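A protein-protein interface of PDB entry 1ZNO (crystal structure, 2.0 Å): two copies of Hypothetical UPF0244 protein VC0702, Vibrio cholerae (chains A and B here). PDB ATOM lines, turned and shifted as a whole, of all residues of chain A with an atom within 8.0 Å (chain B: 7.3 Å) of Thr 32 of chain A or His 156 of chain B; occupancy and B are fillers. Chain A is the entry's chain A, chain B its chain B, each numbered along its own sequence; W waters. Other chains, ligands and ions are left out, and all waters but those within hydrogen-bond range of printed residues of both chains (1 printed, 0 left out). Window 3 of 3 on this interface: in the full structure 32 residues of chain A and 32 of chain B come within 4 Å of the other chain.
Printed residues of chain B that touch a printed residue of chain A: Leu 152, Thr 153, Arg 154, His 156, Leu 157 and Thr 161.
Of the 18 printed residues of chain A, 6 touch a printed residue of chain B.
Hydrophobic or aromatic side chains of chain A that line the printed part of chain B: Ile 168, Leu 169 and Ile 175.
O of Ile 149 of chain B sits at hydrogen-bond distance from OG1 of Thr 153 of chain B (2.8 Å).
The side-chain hydroxyl of Thr 153 of chain B lies within hydrogen-bond range of the backbone NH of His 156 of chain B, at 3.3 Å.
OG1 of Thr 153 of chain B lies within hydrogen-bond range of N of Leu 157 of chain B.
The backbone carbonyl oxygen (O) of Ser 28 of chain A lies within hydrogen-bond range of the side-chain hydroxyl (OG1) of Thr 32 of chain A, 2.9 Å away.
The side-chain hydroxyl of Thr 158 of chain B is in hydrogen-bond range of the backbone NH of Thr 161 of chain B.
Water W1 lies within hydrogen-bond range of NE2 of His 156 of chain B, O of Val 33 of chain A and NH1 of Arg 154 of chain B.
Of chain B, only His 156 (3.2 Å) comes within 4 Å of Thr 32 of chain A.
His 156 of chain B touches just these residues of chain A: Thr 32 (3.2 Å) and Val 33 (3.9 Å).
Printed residues of chain A within 4 Å of Leu 157 of chain B: Gln 165 (3.4 Å), Ile 168 (3.7 Å) and Leu 169 (3.6 Å).
Printed residues of chain A within 4 Å of Thr 161 of chain B: Gln 165 (2.9 Å).
Printed residues of chain B within 4 Å of Val 33 of chain A: Arg 154 (3.6 Å) and His 156 (3.9 Å).
His 155 of chain B touches none of the printed residues of chain A.
Val 26 of chain A touches none of the printed residues of chain B.
The nearest residue of chain B that does not touch Thr 32 of chain A is Arg 154 of chain B (6.9 Å).
The nearest residue of chain A that does not touch His 156 of chain B is Ile 168 of chain A (4.2 Å).
The nearest printed residue of chain A that does not touch Leu 152 of chain B is Leu 171 of chain A (6.1 Å).
The backbone carbonyl oxygen of Thr 32 of chain A sits close to a ring nitrogen (NE2) of His 156 of chain B (3.3 Å).
The side-chain amide nitrogen (NE2) of Gln 165 of chain A is in hydrogen-bond range of the backbone carbonyl oxygen (O) of Thr 161 of chain B.
No position is printed for both chains.
Of the 11 pairs that touch across the chains among the printed residues, none has its exchanged pair printed and touching as well.
Arg 154 of chain B touches Val 33 of chain A (NH1 to O, 3.6 Å).
His 156 of chain B touches Val 33 of chain A (CD2 to CA, 3.9 Å).
O of Gln 165 of chain A touches CD1 of Leu 157 of chain B, at 3.4 Å.
CG2 of Ile 168 of chain A touches CG2 of Thr 153 of chain B, at 3.99 Å.
CB of Ile 168 of chain A touches CD1 of Leu 157 of chain B, at 3.7 Å.
Thr 153 of chain B touches Leu 169 of chain A.
Leu 169 of chain A touches Leu 157 of chain B (CD2 to CD1, 3.6 Å).
Ile 175 of chain A touches Leu 152 of chain B.
CG2 of Ile 175 of chain A touches NE of Arg 154 of chain B, at 3.4 Å.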
ATOM      1  N   ALA A  25      21.643 -35.983  -9.254  1.00  0.00           N
ATOM      2  CA  ALA A  25      22.471 -35.148  -8.398  1.00  0.00           C
ATOM      3  C   ALA A  25      21.930 -33.722  -8.331  1.00  0.00           C
ATOM      4  O   ALA A  25      21.865 -33.131  -7.254  1.00  0.00           O
ATOM      5  CB  ALA A  25      23.907 -35.151  -8.896  1.00  0.00           C
ATOM      6  N   VAL A  26      21.535 -33.169  -9.474  1.00  0.00           N
ATOM      7  CA  VAL A  26      20.996 -31.816  -9.485  1.00  0.00           C
ATOM      8  C   VAL A  26      19.719 -31.747  -8.636  1.00  0.00           C
ATOM      9  O   VAL A  26      19.496 -30.773  -7.913  1.00  0.00           O
ATOM     10  CB  VAL A  26      20.710 -31.336 -10.925  1.00  0.00           C
ATOM     11  CG1 VAL A  26      20.002 -29.986 -10.896  1.00  0.00           C
ATOM     12  CG2 VAL A  26      22.025 -31.201 -11.693  1.00  0.00           C
ATOM     13  N   ARG A  27      18.892 -32.790  -8.715  1.00  0.00           N
ATOM     14  CA  ARG A  27      17.653 -32.855  -7.942  1.00  0.00           C
ATOM     15  C   ARG A  27      17.956 -32.850  -6.445  1.00  0.00           C
ATOM     16  O   ARG A  27      17.422 -32.035  -5.696  1.00  0.00           O
ATOM     17  CB  ARG A  27      16.859 -34.128  -8.267  1.00  0.00           C
ATOM     18  CG  ARG A  27      16.069 -34.113  -9.574  1.00  0.00           C
ATOM     19  CD  ARG A  27      14.882 -35.073  -9.471  1.00  0.00           C
ATOM     20  NE  ARG A  27      14.041 -35.065 -10.664  1.00  0.00           N
ATOM     21  CZ  ARG A  27      14.292 -35.762 -11.768  1.00  0.00           C
ATOM     22  NH1 ARG A  27      15.366 -36.538 -11.836  1.00  0.00           N
ATOM     23  NH2 ARG A  27      13.470 -35.680 -12.806  1.00  0.00           N
ATOM     24  N   SER A  28      18.817 -33.772  -6.026  1.00  0.00           N
ATOM     25  CA  SER A  28      19.202 -33.900  -4.627  1.00  0.00           C
ATOM     26  C   SER A  28      19.807 -32.610  -4.075  1.00  0.00           C
ATOM     27  O   SER A  28      19.516 -32.215  -2.947  1.00  0.00           O
ATOM     28  CB  SER A  28      20.201 -35.046  -4.469  1.00  0.00           C
ATOM     29  OG  SER A  28      20.546 -35.235  -3.107  1.00  0.00           O
ATOM     30  N   ALA A  29      20.650 -31.958  -4.870  1.00  0.00           N
ATOM     31  CA  ALA A  29      21.277 -30.716  -4.442  1.00  0.00           C
ATOM     32  C   ALA A  29      20.212 -29.661  -4.168  1.00  0.00           C
ATOM     33  O   ALA A  29      20.154 -29.097  -3.076  1.00  0.00           O
ATOM     34  CB  ALA A  29      22.249 -30.215  -5.508  1.00  0.00           C
ATOM     35  N   PHE A  30      19.367 -29.395  -5.160  1.00  0.00           N
ATOM     36  CA  PHE A  30      18.313 -28.402  -4.997  1.00  0.00           C
ATOM     37  C   PHE A  30      17.317 -28.749  -3.902  1.00  0.00           C
ATOM     38  O   PHE A  30      16.811 -27.860  -3.217  1.00  0.00           O
ATOM     39  CB  PHE A  30      17.548 -28.191  -6.305  1.00  0.00           C
ATOM     40  CG  PHE A  30      18.198 -27.214  -7.235  1.00  0.00           C
ATOM     41  CD1 PHE A  30      19.220 -27.617  -8.087  1.00  0.00           C
ATOM     42  CD2 PHE A  30      17.785 -25.888  -7.261  1.00  0.00           C
ATOM     43  CE1 PHE A  30      19.825 -26.708  -8.950  1.00  0.00           C
ATOM     44  CE2 PHE A  30      18.384 -24.970  -8.120  1.00  0.00           C
ATOM     45  CZ  PHE A  30      19.404 -25.383  -8.970  1.00  0.00           C
ATOM     46  N   SER A  31      17.021 -30.031  -3.734  1.00  0.00           N
ATOM     47  CA  SER A  31      16.071 -30.426  -2.701  1.00  0.00           C
ATOM     48  C   SER A  31      16.691 -30.224  -1.324  1.00  0.00           C
ATOM     49  O   SER A  31      15.986 -29.955  -0.356  1.00  0.00           O
ATOM     50  CB  SER A  31      15.651 -31.890  -2.876  1.00  0.00           C
ATOM     51  OG  SER A  31      16.716 -32.775  -2.587  1.00  0.00           O
ATOM     52  N   THR A  32      18.013 -30.337  -1.243  1.00  0.00           N
ATOM     53  CA  THR A  32      18.704 -30.165   0.028  1.00  0.00           C
ATOM     54  C   THR A  32      18.771 -28.700   0.429  1.00  0.00           C
ATOM     55  O   THR A  32      18.516 -28.351   1.577  1.00  0.00           O
ATOM     56  CB  THR A  32      20.143 -30.709  -0.032  1.00  0.00           C
ATOM     57  OG1 THR A  32      20.115 -32.140  -0.103  1.00  0.00           O
ATOM     58  CG2 THR A  32      20.925 -30.281   1.200  1.00  0.00           C
ATOM     59  N   VAL A  33      19.118 -27.844  -0.524  1.00  0.00           N
ATOM     60  CA  VAL A  33      19.229 -26.419  -0.261  1.00  0.00           C
ATOM     61  C   VAL A  33      17.846 -25.777  -0.138  1.00  0.00           C
ATOM     62  O   VAL A  33      17.660 -24.828   0.621  1.00  0.00           O
ATOM     63  CB  VAL A  33      20.052 -25.740  -1.373  1.00  0.00           C
ATOM     64  CG1 VAL A  33      20.113 -24.244  -1.153  1.00  0.00           C
ATOM     65  CG2 VAL A  33      21.456 -26.328  -1.392  1.00  0.00           C
ATOM     66  N   PHE A  34      16.880 -26.313  -0.878  1.00  0.00           N
ATOM     67  CA  PHE A  34      15.507 -25.817  -0.842  1.00  0.00           C
ATOM     68  C   PHE A  34      14.584 -26.978  -0.472  1.00  0.00           C
ATOM     69  O   PHE A  34      13.982 -27.614  -1.342  1.00  0.00           O
ATOM     70  CB  PHE A  34      15.120 -25.246  -2.206  1.00  0.00           C
ATOM     71  CG  PHE A  34      16.117 -24.266  -2.754  1.00  0.00           C
ATOM     72  CD1 PHE A  34      17.027 -24.650  -3.734  1.00  0.00           C
ATOM     73  CD2 PHE A  34      16.168 -22.961  -2.272  1.00  0.00           C
ATOM     74  CE1 PHE A  34      17.970 -23.745  -4.228  1.00  0.00           C
ATOM     75  CE2 PHE A  34      17.107 -22.053  -2.759  1.00  0.00           C
ATOM     76  CZ  PHE A  34      18.010 -22.446  -3.739  1.00  0.00           C
ATOM     77  N   PRO A  35      14.460 -27.265   0.836  1.00  0.00           N
ATOM     78  CA  PRO A  35      13.618 -28.354   1.345  1.00  0.00           C
ATOM     79  C   PRO A  35      12.176 -28.295   0.851  1.00  0.00           C
ATOM     80  O   PRO A  35      11.506 -29.323   0.745  1.00  0.00           O
ATOM     81  CB  PRO A  35      13.732 -28.194   2.860  1.00  0.00           C
ATOM     82  CG  PRO A  35      13.922 -26.719   3.024  1.00  0.00           C
ATOM     83  CD  PRO A  35      14.923 -26.408   1.941  1.00  0.00           C
ATOM     84  N   ASP A  36      11.707 -27.089   0.547  1.00  0.00           N
ATOM     85  CA  ASP A  36      10.349 -26.896   0.053  1.00  0.00           C
ATOM     86  C   ASP A  36      10.343 -26.521  -1.428  1.00  0.00           C
ATOM     87  O   ASP A  36      11.018 -27.159  -2.237  1.00  0.00           O
ATOM     88  CB  ASP A  36       9.636 -25.816   0.876  1.00  0.00           C
ATOM     89  CG  ASP A  36      10.498 -24.594   1.104  1.00  0.00           C
ATOM     90  OD1 ASP A  36      11.058 -24.063   0.119  1.00  0.00           O
ATOM     91  OD2 ASP A  36      10.610 -24.160   2.273  1.00  0.00           O
ATOM     92  N   HIS A 164      27.609 -33.935  -5.130  1.00  0.00           N
ATOM     93  CA  HIS A 164      26.640 -33.268  -4.259  1.00  0.00           C
ATOM     94  C   HIS A 164      27.199 -32.027  -3.552  1.00  0.00           C
ATOM     95  O   HIS A 164      26.516 -31.009  -3.436  1.00  0.00           O
ATOM     96  CB  HIS A 164      26.111 -34.245  -3.199  1.00  0.00           C
ATOM     97  CG  HIS A 164      25.027 -33.672  -2.331  1.00  0.00           C
ATOM     98  ND1 HIS A 164      23.774 -33.359  -2.813  1.00  0.00           N
ATOM     99  CD2 HIS A 164      25.012 -33.359  -1.014  1.00  0.00           C
ATOM    100  CE1 HIS A 164      23.033 -32.879  -1.828  1.00  0.00           C
ATOM    101  NE2 HIS A 164      23.760 -32.869  -0.725  1.00  0.00           N
ATOM    102  N   GLN A 165      28.429 -32.112  -3.060  1.00  0.00           N
ATOM    103  CA  GLN A 165      29.023 -30.975  -2.363  1.00  0.00           C
ATOM    104  C   GLN A 165      29.334 -29.824  -3.317  1.00  0.00           C
ATOM    105  O   GLN A 165      29.097 -28.659  -2.998  1.00  0.00           O
ATOM    106  CB  GLN A 165      30.300 -31.398  -1.636  1.00  0.00           C
ATOM    107  CG  GLN A 165      30.092 -32.407  -0.512  1.00  0.00           C
ATOM    108  CD  GLN A 165      31.183 -32.299   0.547  1.00  0.00           C
ATOM    109  OE1 GLN A 165      32.251 -31.735   0.292  1.00  0.00           O
ATOM    110  NE2 GLN A 165      30.920 -32.841   1.737  1.00  0.00           N
ATOM    111  N   ILE A 168      26.122 -27.951  -4.212  1.00  0.00           N
ATOM    112  CA  ILE A 168      25.656 -27.070  -3.140  1.00  0.00           C
ATOM    113  C   ILE A 168      26.475 -25.784  -3.148  1.00  0.00           C
ATOM    114  O   ILE A 168      25.935 -24.679  -3.021  1.00  0.00           O
ATOM    115  CB  ILE A 168      25.809 -27.733  -1.746  1.00  0.00           C
ATOM    116  CG1 ILE A 168      24.989 -29.019  -1.681  1.00  0.00           C
ATOM    117  CG2 ILE A 168      25.380 -26.769  -0.656  1.00  0.00           C
ATOM    118  CD1 ILE A 168      23.520 -28.837  -1.955  1.00  0.00           C
ATOM    119  N   LEU A 169      27.787 -25.933  -3.294  1.00  0.00           N
ATOM    120  CA  LEU A 169      28.687 -24.785  -3.323  1.00  0.00           C
ATOM    121  C   LEU A 169      28.391 -23.883  -4.507  1.00  0.00           C
ATOM    122  O   LEU A 169      28.532 -22.664  -4.422  1.00  0.00           O
ATOM    123  CB  LEU A 169      30.142 -25.253  -3.396  1.00  0.00           C
ATOM    124  CG  LEU A 169      30.617 -25.986  -2.146  1.00  0.00           C
ATOM    125  CD1 LEU A 169      32.033 -26.484  -2.366  1.00  0.00           C
ATOM    126  CD2 LEU A 169      30.556 -25.038  -0.940  1.00  0.00           C
ATOM    127  N   LEU A 171      25.575 -23.286  -5.597  1.00  0.00           N
ATOM    128  CA  LEU A 171      24.331 -22.580  -5.317  1.00  0.00           C
ATOM    129  C   LEU A 171      24.481 -21.380  -4.378  1.00  0.00           C
ATOM    130  O   LEU A 171      23.523 -20.640  -4.154  1.00  0.00           O
ATOM    131  CB  LEU A 171      23.293 -23.554  -4.749  1.00  0.00           C
ATOM    132  CG  LEU A 171      22.409 -24.270  -5.778  1.00  0.00           C
ATOM    133  CD1 LEU A 171      23.249 -24.902  -6.869  1.00  0.00           C
ATOM    134  CD2 LEU A 171      21.579 -25.331  -5.063  1.00  0.00           C
ATOM    135  N   ILE A 175      21.849 -18.512  -2.659  1.00  0.00           N
ATOM    136  CA  ILE A 175      21.493 -18.700  -1.257  1.00  0.00           C
ATOM    137  C   ILE A 175      21.709 -17.393  -0.487  1.00  0.00           C
ATOM    138  O   ILE A 175      21.064 -17.150   0.532  1.00  0.00           O
ATOM    139  CB  ILE A 175      22.382 -19.803  -0.586  1.00  0.00           C
ATOM    140  CG1 ILE A 175      22.109 -21.175  -1.200  1.00  0.00           C
ATOM    141  CG2 ILE A 175      22.104 -19.865   0.907  1.00  0.00           C
ATOM    142  CD1 ILE A 175      22.966 -22.300  -0.598  1.00  0.00           C
ATOM    143  N   ILE B 149      32.198 -21.748   4.755  1.00  0.00           N
ATOM    144  CA  ILE B 149      31.381 -22.722   4.032  1.00  0.00           C
ATOM    145  C   ILE B 149      30.039 -22.961   4.723  1.00  0.00           C
ATOM    146  O   ILE B 149      28.981 -22.914   4.090  1.00  0.00           O
ATOM    147  CB  ILE B 149      32.119 -24.066   3.905  1.00  0.00           C
ATOM    148  CG1 ILE B 149      33.251 -23.932   2.880  1.00  0.00           C
ATOM    149  CG2 ILE B 149      31.132 -25.177   3.523  1.00  0.00           C
ATOM    150  CD1 ILE B 149      34.185 -25.133   2.829  1.00  0.00           C
ATOM    151  N   GLY B 150      30.091 -23.222   6.025  1.00  0.00           N
ATOM    152  CA  GLY B 150      28.874 -23.468   6.771  1.00  0.00           C
ATOM    153  C   GLY B 150      27.915 -22.294   6.728  1.00  0.00           C
ATOM    154  O   GLY B 150      26.704 -22.463   6.574  1.00  0.00           O
ATOM    155  N   LEU B 151      28.457 -21.088   6.856  1.00  0.00           N
ATOM    156  CA  LEU B 151      27.627 -19.894   6.841  1.00  0.00           C
ATOM    157  C   LEU B 151      27.021 -19.673   5.459  1.00  0.00           C
ATOM    158  O   LEU B 151      25.815 -19.465   5.329  1.00  0.00           O
ATOM    159  CB  LEU B 151      28.457 -18.680   7.280  1.00  0.00           C
ATOM    160  CG  LEU B 151      27.775 -17.325   7.511  1.00  0.00           C
ATOM    161  CD1 LEU B 151      27.541 -16.638   6.181  1.00  0.00           C
ATOM    162  CD2 LEU B 151      26.475 -17.509   8.270  1.00  0.00           C
ATOM    163  N   LEU B 152      27.853 -19.758   4.426  1.00  0.00           N
ATOM    164  CA  LEU B 152      27.403 -19.549   3.055  1.00  0.00           C
ATOM    165  C   LEU B 152      26.462 -20.618   2.495  1.00  0.00           C
ATOM    166  O   LEU B 152      25.705 -20.341   1.563  1.00  0.00           O
ATOM    167  CB  LEU B 152      28.624 -19.376   2.143  1.00  0.00           C
ATOM    168  CG  LEU B 152      29.492 -18.147   2.457  1.00  0.00           C
ATOM    169  CD1 LEU B 152      30.819 -18.228   1.715  1.00  0.00           C
ATOM    170  CD2 LEU B 152      28.737 -16.876   2.069  1.00  0.00           C
ATOM    171  N   THR B 153      26.497 -21.832   3.048  1.00  0.00           N
ATOM    172  CA  THR B 153      25.617 -22.913   2.567  1.00  0.00           C
ATOM    173  C   THR B 153      24.455 -23.213   3.518  1.00  0.00           C
ATOM    174  O   THR B 153      23.840 -24.277   3.431  1.00  0.00           O
ATOM    175  CB  THR B 153      26.378 -24.260   2.371  1.00  0.00           C
ATOM    176  OG1 THR B 153      26.870 -24.723   3.637  1.00  0.00           O
ATOM    177  CG2 THR B 153      27.531 -24.108   1.390  1.00  0.00           C
ATOM    178  N   ARG B 154      24.151 -22.281   4.414  1.00  0.00           N
ATOM    179  CA  ARG B 154      23.073 -22.490   5.382  1.00  0.00           C
ATOM    180  C   ARG B 154      23.340 -23.788   6.130  1.00  0.00           C
ATOM    181  O   ARG B 154      22.413 -24.520   6.478  1.00  0.00           O
ATOM    182  CB  ARG B 154      21.708 -22.596   4.691  1.00  0.00           C
ATOM    183  CG  ARG B 154      21.194 -21.322   4.035  1.00  0.00           C
ATOM    184  CD  ARG B 154      19.746 -21.519   3.602  1.00  0.00           C
ATOM    185  NE  ARG B 154      19.282 -20.494   2.666  1.00  0.00           N
ATOM    186  CZ  ARG B 154      18.127 -20.550   2.006  1.00  0.00           C
ATOM    187  NH1 ARG B 154      17.307 -21.580   2.177  1.00  0.00           N
ATOM    188  NH2 ARG B 154      17.794 -19.582   1.165  1.00  0.00           N
ATOM    189  N   HIS B 155      24.621 -24.071   6.347  1.00  0.00           N
ATOM    190  CA  HIS B 155      25.067 -25.262   7.054  1.00  0.00           C
ATOM    191  C   HIS B 155      24.743 -26.563   6.313  1.00  0.00           C
ATOM    192  O   HIS B 155      24.736 -27.626   6.905  1.00  0.00           O
ATOM    193  CB  HIS B 155      24.472 -25.287   8.469  1.00  0.00           C
ATOM    194  CG  HIS B 155      25.393 -25.866   9.501  1.00  0.00           C
ATOM    195  ND1 HIS B 155      25.496 -27.222   9.736  1.00  0.00           N
ATOM    196  CD2 HIS B 155      26.256 -25.272  10.355  1.00  0.00           C
ATOM    197  CE1 HIS B 155      26.381 -27.436  10.693  1.00  0.00           C
ATOM    198  NE2 HIS B 155      26.859 -26.270  11.089  1.00  0.00           N
ATOM    199  N   HIS B 156      24.466 -26.489   5.020  1.00  0.00           N
ATOM    200  CA  HIS B 156      24.217 -27.725   4.319  1.00  0.00           C
ATOM    201  C   HIS B 156      25.577 -28.381   4.086  1.00  0.00           C
ATOM    202  O   HIS B 156      25.691 -29.572   3.798  1.00  0.00           O
ATOM    203  CB  HIS B 156      23.417 -27.475   3.046  1.00  0.00           C
ATOM    204  CG  HIS B 156      21.985 -27.127   3.328  1.00  0.00           C
ATOM    205  ND1 HIS B 156      21.169 -27.938   4.080  1.00  0.00           N
ATOM    206  CD2 HIS B 156      21.255 -26.026   3.026  1.00  0.00           C
ATOM    207  CE1 HIS B 156      19.988 -27.352   4.234  1.00  0.00           C
ATOM    208  NE2 HIS B 156      20.018 -26.195   3.607  1.00  0.00           N
ATOM    209  N   LEU B 157      26.617 -27.582   4.254  1.00  0.00           N
ATOM    210  CA  LEU B 157      27.978 -28.060   4.153  1.00  0.00           C
ATOM    211  C   LEU B 157      28.713 -27.326   5.255  1.00  0.00           C
ATOM    212  O   LEU B 157      28.243 -26.301   5.743  1.00  0.00           O
ATOM    213  CB  LEU B 157      28.610 -27.705   2.803  1.00  0.00           C
ATOM    214  CG  LEU B 157      28.120 -28.434   1.550  1.00  0.00           C
ATOM    215  CD1 LEU B 157      28.889 -27.922   0.321  1.00  0.00           C
ATOM    216  CD2 LEU B 157      28.331 -29.936   1.712  1.00  0.00           C
ATOM    217  N   THR B 158      29.841 -27.874   5.675  1.00  0.00           N
ATOM    218  CA  THR B 158      30.656 -27.226   6.682  1.00  0.00           C
ATOM    219  C   THR B 158      32.068 -27.430   6.195  1.00  0.00           C
ATOM    220  O   THR B 158      32.320 -28.255   5.304  1.00  0.00           O
ATOM    221  CB  THR B 158      30.533 -27.867   8.084  1.00  0.00           C
ATOM    222  OG1 THR B 158      31.096 -29.185   8.066  1.00  0.00           O
ATOM    223  CG2 THR B 158      29.076 -27.934   8.517  1.00  0.00           C
ATOM    224  N   THR B 161      33.005 -31.076   6.740  1.00  0.00           N
ATOM    225  CA  THR B 161      32.529 -32.078   5.796  1.00  0.00           C
ATOM    226  C   THR B 161      33.132 -31.914   4.400  1.00  0.00           C
ATOM    227  O   THR B 161      33.171 -32.865   3.630  1.00  0.00           O
ATOM    228  CB  THR B 161      30.984 -32.100   5.716  1.00  0.00           C
ATOM    229  OG1 THR B 161      30.487 -30.847   5.224  1.00  0.00           O
ATOM    230  CG2 THR B 161      30.399 -32.377   7.101  1.00  0.00           C
HETATM  231  O   HOH W   1      18.519 -24.015   3.070  1.00  0.00           O
